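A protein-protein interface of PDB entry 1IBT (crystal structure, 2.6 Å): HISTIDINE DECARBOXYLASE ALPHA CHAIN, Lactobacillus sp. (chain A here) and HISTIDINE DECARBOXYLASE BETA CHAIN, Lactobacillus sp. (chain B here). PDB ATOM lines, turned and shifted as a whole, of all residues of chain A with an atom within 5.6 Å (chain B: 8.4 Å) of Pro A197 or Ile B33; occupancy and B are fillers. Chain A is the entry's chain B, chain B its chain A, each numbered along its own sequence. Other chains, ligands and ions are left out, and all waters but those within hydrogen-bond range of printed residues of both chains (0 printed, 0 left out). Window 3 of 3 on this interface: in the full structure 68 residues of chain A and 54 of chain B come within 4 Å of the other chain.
Printed residues of chain A that touch a printed residue of chain B: Ile A194, Pro A197, Asp A198, Asp A200 and Met A201. Hydrophobic or aromatic side chains of chain A within 4 Å of the printed part of chain B: Ile A194, Pro A197 and Met A201. Hydrophobic or aromatic side chains of chain B within 4 Å of the printed part of chain A: Ile B15, Ile B17 and Ile B33. Among the printed residues, no Asp or Glu carboxylate lies within 4 Å of a Lys or Arg side-chain nitrogen of the other chain.
Of the printed residues of chain B, Ile A194 touches Ile B33. Pro A197 touches just these residues of chain B: Ile B15 and Ile B33. Of the printed residues of chain B, Asp A200 touches Ile B17. Printed residues of chain A within 4 Å of Arg B14: Met A201. Of the printed residues of chain A, Ile B15 touches Pro A197 (3.7 Å), Asp A198 (3.96 Å) and Met A201 (3.7 Å). Of the printed residues of chain A, Ala B16 touches Met A201. Of the printed residues of chain A, Ile B33 touches Ile A194 and Pro A197. Gly B36 touches none of the printed residues of chain A. The nearest residue of chain B that does not touch Pro A197 is Ile B17 (4.5 Å). The nearest printed residue of chain A that does not touch Ile B33 is Leu A195 (6.3 Å). The nearest printed residue of chain B that does not touch Ile A194 is Ile B17 (4.3 Å).
SD of Met A201 is in hydrogen-bond range of N of Ala B16.
Among the printed residues, pairs that only touch across the chains: Ile A194 with Ile B33 (3.7 Å), Pro A197 with Ile B15 (3.7 Å), Pro A197 with Ile B33 (3.7 Å), Asp A198 with Ile B15 (3.96 Å), Asp A200 with Ile B17 (3.8 Å), Met A201 with Arg B14 (3.7 Å), Met A201 with Ile B15 (3.7 Å) and Met A201 with Ile B17 (3.8 Å).
OD1 of Asp B13 sits at hydrogen-bond distance from N of Ile B15. The backbone carbonyl oxygen (O) of Ile B15 is in hydrogen-bond range of the backbone NH (N) of Asn B35 (3.0 Å). The backbone carbonyl oxygen of Ile B15 lies within hydrogen-bond range of the backbone NH of Gly B36. The backbone NH of Ile B17 lies within hydrogen-bond range of the backbone carbonyl oxygen of Ile B33 (2.7 Å). N of Ser A193 sits at hydrogen-bond distance from OD1 of Asp A200 (2.9 Å). OD1 of Asp A200 lies within hydrogen-bond range of OG1 of Thr A196 (3.5 Å).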
ATOM      1  N   SER A 193      -3.302 -10.875  33.520  1.00  0.00           N
ATOM      2  CA  SER A 193      -2.447  -9.759  33.801  1.00  0.00           C
ATOM      3  C   SER A 193      -2.550  -8.786  32.673  1.00  0.00           C
ATOM      4  O   SER A 193      -2.636  -9.174  31.526  1.00  0.00           O
ATOM      5  CB  SER A 193      -1.009 -10.222  33.932  1.00  0.00           C
ATOM      6  OG  SER A 193      -0.114  -9.161  34.228  1.00  0.00           O
ATOM      7  N   ILE A 194      -2.353  -7.507  32.968  1.00  0.00           N
ATOM      8  CA  ILE A 194      -2.456  -6.503  31.940  1.00  0.00           C
ATOM      9  C   ILE A 194      -1.328  -6.656  30.930  1.00  0.00           C
ATOM     10  O   ILE A 194      -1.275  -6.022  29.884  1.00  0.00           O
ATOM     11  CB  ILE A 194      -2.498  -5.170  32.717  1.00  0.00           C
ATOM     12  CG1 ILE A 194      -2.865  -4.061  31.795  1.00  0.00           C
ATOM     13  CG2 ILE A 194      -1.198  -4.890  33.358  1.00  0.00           C
ATOM     14  CD1 ILE A 194      -4.387  -3.987  31.630  1.00  0.00           C
ATOM     15  N   LEU A 195      -0.370  -7.517  31.224  1.00  0.00           N
ATOM     16  CA  LEU A 195       0.732  -7.753  30.317  1.00  0.00           C
ATOM     17  C   LEU A 195       0.563  -9.033  29.520  1.00  0.00           C
ATOM     18  O   LEU A 195       1.408  -9.277  28.668  1.00  0.00           O
ATOM     19  CB  LEU A 195       2.040  -7.828  31.099  1.00  0.00           C
ATOM     20  CG  LEU A 195       2.565  -6.600  31.789  1.00  0.00           C
ATOM     21  CD1 LEU A 195       3.621  -7.014  32.752  1.00  0.00           C
ATOM     22  CD2 LEU A 195       3.115  -5.627  30.786  1.00  0.00           C
ATOM     23  N   THR A 196      -0.469  -9.844  29.764  1.00  0.00           N
ATOM     24  CA  THR A 196      -0.671 -11.086  29.054  1.00  0.00           C
ATOM     25  C   THR A 196      -1.976 -11.163  28.272  1.00  0.00           C
ATOM     26  O   THR A 196      -2.682 -12.169  28.356  1.00  0.00           O
ATOM     27  CB  THR A 196      -0.613 -12.259  30.038  1.00  0.00           C
ATOM     28  OG1 THR A 196      -1.401 -11.927  31.161  1.00  0.00           O
ATOM     29  CG2 THR A 196       0.804 -12.613  30.394  1.00  0.00           C
ATOM     30  N   PRO A 197      -2.341 -10.173  27.461  1.00  0.00           N
ATOM     31  CA  PRO A 197      -3.670 -10.013  26.912  1.00  0.00           C
ATOM     32  C   PRO A 197      -4.204 -11.259  26.256  1.00  0.00           C
ATOM     33  O   PRO A 197      -5.309 -11.705  26.568  1.00  0.00           O
ATOM     34  CB  PRO A 197      -3.550  -8.865  25.942  1.00  0.00           C
ATOM     35  CG  PRO A 197      -2.357  -8.101  26.449  1.00  0.00           C
ATOM     36  CD  PRO A 197      -1.442  -9.258  26.784  1.00  0.00           C
ATOM     37  N   ASP A 198      -3.421 -11.930  25.409  1.00  0.00           N
ATOM     38  CA  ASP A 198      -4.007 -13.001  24.645  1.00  0.00           C
ATOM     39  C   ASP A 198      -4.190 -14.226  25.510  1.00  0.00           C
ATOM     40  O   ASP A 198      -5.222 -14.901  25.405  1.00  0.00           O
ATOM     41  CB  ASP A 198      -3.144 -13.267  23.423  1.00  0.00           C
ATOM     42  CG  ASP A 198      -1.773 -13.891  23.598  1.00  0.00           C
ATOM     43  OD1 ASP A 198      -1.753 -15.137  23.645  1.00  0.00           O
ATOM     44  OD2 ASP A 198      -0.765 -13.154  23.581  1.00  0.00           O
ATOM     45  N   LYS A 199      -3.317 -14.420  26.484  1.00  0.00           N
ATOM     46  CA  LYS A 199      -3.476 -15.507  27.415  1.00  0.00           C
ATOM     47  C   LYS A 199      -4.682 -15.236  28.246  1.00  0.00           C
ATOM     48  O   LYS A 199      -5.347 -16.200  28.621  1.00  0.00           O
ATOM     49  CB  LYS A 199      -2.324 -15.619  28.361  1.00  0.00           C
ATOM     50  CG  LYS A 199      -2.254 -16.860  29.213  1.00  0.00           C
ATOM     51  CD  LYS A 199      -1.497 -16.465  30.480  1.00  0.00           C
ATOM     52  CE  LYS A 199      -0.941 -17.706  31.123  1.00  0.00           C
ATOM     53  NZ  LYS A 199       0.090 -18.230  30.232  1.00  0.00           N
ATOM     54  N   ASP A 200      -4.991 -13.976  28.573  1.00  0.00           N
ATOM     55  CA  ASP A 200      -6.173 -13.632  29.387  1.00  0.00           C
ATOM     56  C   ASP A 200      -7.460 -14.153  28.789  1.00  0.00           C
ATOM     57  O   ASP A 200      -8.306 -14.745  29.463  1.00  0.00           O
ATOM     58  CB  ASP A 200      -6.339 -12.158  29.518  1.00  0.00           C
ATOM     59  CG  ASP A 200      -5.253 -11.439  30.255  1.00  0.00           C
ATOM     60  OD1 ASP A 200      -4.850 -11.859  31.316  1.00  0.00           O
ATOM     61  OD2 ASP A 200      -4.775 -10.438  29.785  1.00  0.00           O
ATOM     62  N   MET A 201      -7.581 -13.976  27.474  1.00  0.00           N
ATOM     63  CA  MET A 201      -8.739 -14.467  26.758  1.00  0.00           C
ATOM     64  C   MET A 201      -8.742 -15.974  26.857  1.00  0.00           C
ATOM     65  O   MET A 201      -9.796 -16.516  27.193  1.00  0.00           O
ATOM     66  CB  MET A 201      -8.753 -14.094  25.253  1.00  0.00           C
ATOM     67  CG  MET A 201      -8.721 -12.595  24.909  1.00  0.00           C
ATOM     68  SD  MET A 201      -9.552 -11.556  26.140  1.00  0.00           S
ATOM     69  CE  MET A 201     -11.202 -11.849  25.574  1.00  0.00           C
ATOM     70  N   GLU A 202      -7.617 -16.676  26.671  1.00  0.00           N
ATOM     71  CA  GLU A 202      -7.598 -18.130  26.756  1.00  0.00           C
ATOM     72  C   GLU A 202      -7.947 -18.610  28.149  1.00  0.00           C
ATOM     73  O   GLU A 202      -8.556 -19.665  28.303  1.00  0.00           O
ATOM     74  CB  GLU A 202      -6.239 -18.673  26.364  1.00  0.00           C
ATOM     75  CG  GLU A 202      -6.004 -18.341  24.895  1.00  0.00           C
ATOM     76  CD  GLU A 202      -4.864 -19.060  24.185  1.00  0.00           C
ATOM     77  OE1 GLU A 202      -4.980 -19.389  22.971  1.00  0.00           O
ATOM     78  OE2 GLU A 202      -3.827 -19.293  24.818  1.00  0.00           O
ATOM     79  N   ASP B  13      -7.926 -10.445  15.699  1.00  0.00           N
ATOM     80  CA  ASP B  13      -7.806 -11.014  17.010  1.00  0.00           C
ATOM     81  C   ASP B  13      -9.075 -10.732  17.756  1.00  0.00           C
ATOM     82  O   ASP B  13      -9.872  -9.885  17.383  1.00  0.00           O
ATOM     83  CB  ASP B  13      -6.643 -10.420  17.771  1.00  0.00           C
ATOM     84  CG  ASP B  13      -6.704  -8.969  18.226  1.00  0.00           C
ATOM     85  OD1 ASP B  13      -7.252  -8.738  19.296  1.00  0.00           O
ATOM     86  OD2 ASP B  13      -6.170  -8.093  17.557  1.00  0.00           O
ATOM     87  N   ARG B  14      -9.279 -11.465  18.818  1.00  0.00           N
ATOM     88  CA  ARG B  14     -10.478 -11.326  19.578  1.00  0.00           C
ATOM     89  C   ARG B  14     -10.055 -10.975  20.978  1.00  0.00           C
ATOM     90  O   ARG B  14     -10.575 -11.531  21.948  1.00  0.00           O
ATOM     91  CB  ARG B  14     -11.282 -12.644  19.569  1.00  0.00           C
ATOM     92  CG  ARG B  14     -11.711 -13.142  18.191  1.00  0.00           C
ATOM     93  CD  ARG B  14     -12.763 -14.245  18.245  1.00  0.00           C
ATOM     94  NE  ARG B  14     -12.231 -15.499  18.766  1.00  0.00           N
ATOM     95  CZ  ARG B  14     -12.985 -16.524  19.178  1.00  0.00           C
ATOM     96  NH1 ARG B  14     -14.327 -16.435  19.110  1.00  0.00           N
ATOM     97  NH2 ARG B  14     -12.393 -17.594  19.735  1.00  0.00           N
ATOM     98  N   ILE B  15      -9.093 -10.089  21.160  1.00  0.00           N
ATOM     99  CA  ILE B  15      -8.605  -9.748  22.499  1.00  0.00           C
ATOM    100  C   ILE B  15      -9.385  -8.512  22.900  1.00  0.00           C
ATOM    101  O   ILE B  15      -9.486  -7.598  22.074  1.00  0.00           O
ATOM    102  CB  ILE B  15      -7.086  -9.437  22.457  1.00  0.00           C
ATOM    103  CG1 ILE B  15      -6.299 -10.635  21.958  1.00  0.00           C
ATOM    104  CG2 ILE B  15      -6.612  -9.077  23.853  1.00  0.00           C
ATOM    105  CD1 ILE B  15      -4.887 -10.333  21.416  1.00  0.00           C
ATOM    106  N   ALA B  16      -9.926  -8.471  24.111  1.00  0.00           N
ATOM    107  CA  ALA B  16     -10.742  -7.367  24.530  1.00  0.00           C
ATOM    108  C   ALA B  16     -10.485  -7.132  25.974  1.00  0.00           C
ATOM    109  O   ALA B  16     -11.090  -7.816  26.795  1.00  0.00           O
ATOM    110  CB  ALA B  16     -12.208  -7.684  24.358  1.00  0.00           C
ATOM    111  N   ILE B  17      -9.637  -6.174  26.355  1.00  0.00           N
ATOM    112  CA  ILE B  17      -9.277  -6.033  27.759  1.00  0.00           C
ATOM    113  C   ILE B  17      -9.501  -4.603  28.197  1.00  0.00           C
ATOM    114  O   ILE B  17      -9.176  -3.667  27.474  1.00  0.00           O
ATOM    115  CB  ILE B  17      -7.781  -6.469  27.950  1.00  0.00           C
ATOM    116  CG1 ILE B  17      -7.572  -7.952  27.618  1.00  0.00           C
ATOM    117  CG2 ILE B  17      -7.354  -6.229  29.405  1.00  0.00           C
ATOM    118  CD1 ILE B  17      -8.254  -8.974  28.537  1.00  0.00           C
ATOM    119  N   SER B  18     -10.058  -4.485  29.391  1.00  0.00           N
ATOM    120  CA  SER B  18     -10.401  -3.243  30.041  1.00  0.00           C
ATOM    121  C   SER B  18      -9.241  -2.888  30.967  1.00  0.00           C
ATOM    122  O   SER B  18      -8.765  -3.705  31.773  1.00  0.00           O
ATOM    123  CB  SER B  18     -11.690  -3.435  30.838  1.00  0.00           C
ATOM    124  OG  SER B  18     -12.011  -2.493  31.838  1.00  0.00           O
ATOM    125  N   PRO B  19      -8.763  -1.655  30.916  1.00  0.00           N
ATOM    126  CA  PRO B  19      -7.792  -1.131  31.823  1.00  0.00           C
ATOM    127  C   PRO B  19      -8.247  -0.926  33.239  1.00  0.00           C
ATOM    128  O   PRO B  19      -7.421  -0.617  34.092  1.00  0.00           O
ATOM    129  CB  PRO B  19      -7.377   0.124  31.171  1.00  0.00           C
ATOM    130  CG  PRO B  19      -8.624   0.545  30.511  1.00  0.00           C
ATOM    131  CD  PRO B  19      -9.000  -0.721  29.854  1.00  0.00           C
ATOM    132  N   TYR B  20      -9.519  -1.084  33.553  1.00  0.00           N
ATOM    133  CA  TYR B  20      -9.964  -0.640  34.845  1.00  0.00           C
ATOM    134  C   TYR B  20      -9.992  -1.740  35.832  1.00  0.00           C
ATOM    135  O   TYR B  20      -9.824  -2.921  35.536  1.00  0.00           O
ATOM    136  CB  TYR B  20     -11.354  -0.065  34.780  1.00  0.00           C
ATOM    137  CG  TYR B  20     -11.526   1.197  33.966  1.00  0.00           C
ATOM    138  CD1 TYR B  20     -10.445   1.926  33.504  1.00  0.00           C
ATOM    139  CD2 TYR B  20     -12.811   1.585  33.642  1.00  0.00           C
ATOM    140  CE1 TYR B  20     -10.644   3.036  32.706  1.00  0.00           C
ATOM    141  CE2 TYR B  20     -13.003   2.708  32.842  1.00  0.00           C
ATOM    142  CZ  TYR B  20     -11.920   3.410  32.381  1.00  0.00           C
ATOM    143  OH  TYR B  20     -12.109   4.457  31.537  1.00  0.00           O
ATOM    144  N   ARG B  25     -15.957  -2.341  30.041  1.00  0.00           N
ATOM    145  CA  ARG B  25     -16.234  -1.134  29.340  1.00  0.00           C
ATOM    146  C   ARG B  25     -16.466  -1.455  27.882  1.00  0.00           C
ATOM    147  O   ARG B  25     -16.392  -2.619  27.503  1.00  0.00           O
ATOM    148  CB  ARG B  25     -15.086  -0.174  29.614  1.00  0.00           C
ATOM    149  CG  ARG B  25     -13.682  -0.678  29.691  1.00  0.00           C
ATOM    150  CD  ARG B  25     -12.979   0.458  30.431  1.00  0.00           C
ATOM    151  NE  ARG B  25     -12.258   1.177  29.449  1.00  0.00           N
ATOM    152  CZ  ARG B  25     -11.861   2.315  28.908  1.00  0.00           C
ATOM    153  NH1 ARG B  25     -12.056   3.591  29.138  1.00  0.00           N
ATOM    154  NH2 ARG B  25     -11.014   1.981  27.983  1.00  0.00           N
ATOM    155  N   GLY B  26     -16.786  -0.514  27.035  1.00  0.00           N
ATOM    156  CA  GLY B  26     -17.315  -0.826  25.740  1.00  0.00           C
ATOM    157  C   GLY B  26     -16.282  -0.972  24.696  1.00  0.00           C
ATOM    158  O   GLY B  26     -15.197  -0.428  24.753  1.00  0.00           O
ATOM    159  N   GLU B  29     -13.849   1.835  23.052  1.00  0.00           N
ATOM    160  CA  GLU B  29     -13.439   2.905  23.928  1.00  0.00           C
ATOM    161  C   GLU B  29     -11.916   3.026  24.008  1.00  0.00           C
ATOM    162  O   GLU B  29     -11.240   1.996  23.961  1.00  0.00           O
ATOM    163  CB  GLU B  29     -13.978   2.682  25.320  1.00  0.00           C
ATOM    164  CG  GLU B  29     -15.470   2.675  25.443  1.00  0.00           C
ATOM    165  CD  GLU B  29     -15.969   3.090  26.811  1.00  0.00           C
ATOM    166  OE1 GLU B  29     -16.180   2.290  27.712  1.00  0.00           O
ATOM    167  OE2 GLU B  29     -16.169   4.264  27.015  1.00  0.00           O
ATOM    168  N   PRO B  30     -11.277   4.198  24.148  1.00  0.00           N
ATOM    169  CA  PRO B  30      -9.852   4.363  24.164  1.00  0.00           C
ATOM    170  C   PRO B  30      -9.247   3.734  25.407  1.00  0.00           C
ATOM    171  O   PRO B  30      -9.832   3.737  26.501  1.00  0.00           O
ATOM    172  CB  PRO B  30      -9.676   5.847  24.078  1.00  0.00           C
ATOM    173  CG  PRO B  30     -10.786   6.361  24.950  1.00  0.00           C
ATOM    174  CD  PRO B  30     -11.911   5.478  24.452  1.00  0.00           C
ATOM    175  N   GLY B  31      -8.093   3.096  25.212  1.00  0.00           N
ATOM    176  CA  GLY B  31      -7.353   2.494  26.305  1.00  0.00           C
ATOM    177  C   GLY B  31      -7.669   1.036  26.522  1.00  0.00           C
ATOM    178  O   GLY B  31      -7.159   0.405  27.445  1.00  0.00           O
ATOM    179  N   ASN B  32      -8.571   0.493  25.731  1.00  0.00           N
ATOM    180  CA  ASN B  32      -8.845  -0.916  25.843  1.00  0.00           C
ATOM    181  C   ASN B  32      -7.684  -1.551  25.112  1.00  0.00           C
ATOM    182  O   ASN B  32      -7.120  -0.988  24.161  1.00  0.00           O
ATOM    183  CB  ASN B  32     -10.154  -1.262  25.168  1.00  0.00           C
ATOM    184  CG  ASN B  32     -11.338  -1.155  26.096  1.00  0.00           C
ATOM    185  OD1 ASN B  32     -11.256  -0.791  27.265  1.00  0.00           O
ATOM    186  ND2 ASN B  32     -12.516  -1.441  25.600  1.00  0.00           N
ATOM    187  N   ILE B  33      -7.269  -2.700  25.605  1.00  0.00           N
ATOM    188  CA  ILE B  33      -6.181  -3.445  24.992  1.00  0.00           C
ATOM    189  C   ILE B  33      -6.842  -4.530  24.152  1.00  0.00           C
ATOM    190  O   ILE B  33      -7.706  -5.269  24.632  1.00  0.00           O
ATOM    191  CB  ILE B  33      -5.290  -4.018  26.135  1.00  0.00           C
ATOM    192  CG1 ILE B  33      -4.556  -2.869  26.810  1.00  0.00           C
ATOM    193  CG2 ILE B  33      -4.284  -5.032  25.589  1.00  0.00           C
ATOM    194  CD1 ILE B  33      -3.793  -3.202  28.092  1.00  0.00           C
ATOM    195  N   GLY B  34      -6.509  -4.616  22.890  1.00  0.00           N
ATOM    196  CA  GLY B  34      -7.035  -5.688  22.085  1.00  0.00           C
ATOM    197  C   GLY B  34      -7.887  -5.146  20.986  1.00  0.00           C
ATOM    198  O   GLY B  34      -8.328  -4.009  21.064  1.00  0.00           O
ATOM    199  N   ASN B  35      -8.131  -5.940  19.966  1.00  0.00           N
ATOM    200  CA  ASN B  35      -8.895  -5.486  18.848  1.00  0.00           C
ATOM    201  C   ASN B  35     -10.157  -6.270  18.608  1.00  0.00           C
ATOM    202  O   ASN B  35     -10.739  -6.251  17.525  1.00  0.00           O
ATOM    203  CB  ASN B  35      -8.047  -5.523  17.610  1.00  0.00           C
ATOM    204  CG  ASN B  35      -6.888  -4.555  17.578  1.00  0.00           C
ATOM    205  OD1 ASN B  35      -6.743  -3.682  18.421  1.00  0.00           O
ATOM    206  ND2 ASN B  35      -6.022  -4.660  16.592  1.00  0.00           N
ATOM    207  N   GLY B  36     -10.666  -6.910  19.631  1.00  0.00           N
ATOM    208  CA  GLY B  36     -11.891  -7.676  19.527  1.00  0.00           C
ATOM    209  C   GLY B  36     -12.894  -7.255  20.584  1.00  0.00           C
ATOM    210  O   GLY B  36     -12.679  -6.267  21.280  1.00  0.00           O
ATOM    211  N   TYR B  37     -13.977  -8.017  20.732  1.00  0.00           N
ATOM    212  CA  TYR B  37     -15.058  -7.719  21.667  1.00  0.00           C
ATOM    213  C   TYR B  37     -15.730  -8.942  22.257  1.00  0.00           C
ATOM    214  O   TYR B  37     -15.729 -10.019  21.664  1.00  0.00           O
ATOM    215  CB  TYR B  37     -16.130  -6.875  20.986  1.00  0.00           C
ATOM    216  CG  TYR B  37     -16.702  -7.394  19.686  1.00  0.00           C
ATOM    217  CD1 TYR B  37     -17.563  -8.474  19.675  1.00  0.00           C
ATOM    218  CD2 TYR B  37     -16.404  -6.752  18.497  1.00  0.00           C
ATOM    219  CE1 TYR B  37     -18.129  -8.910  18.486  1.00  0.00           C
ATOM    220  CE2 TYR B  37     -16.974  -7.178  17.300  1.00  0.00           C
ATOM    221  CZ  TYR B  37     -17.836  -8.260  17.309  1.00  0.00           C
ATOM    222  OH  TYR B  37     -18.418  -8.696  16.137  1.00  0.00           O
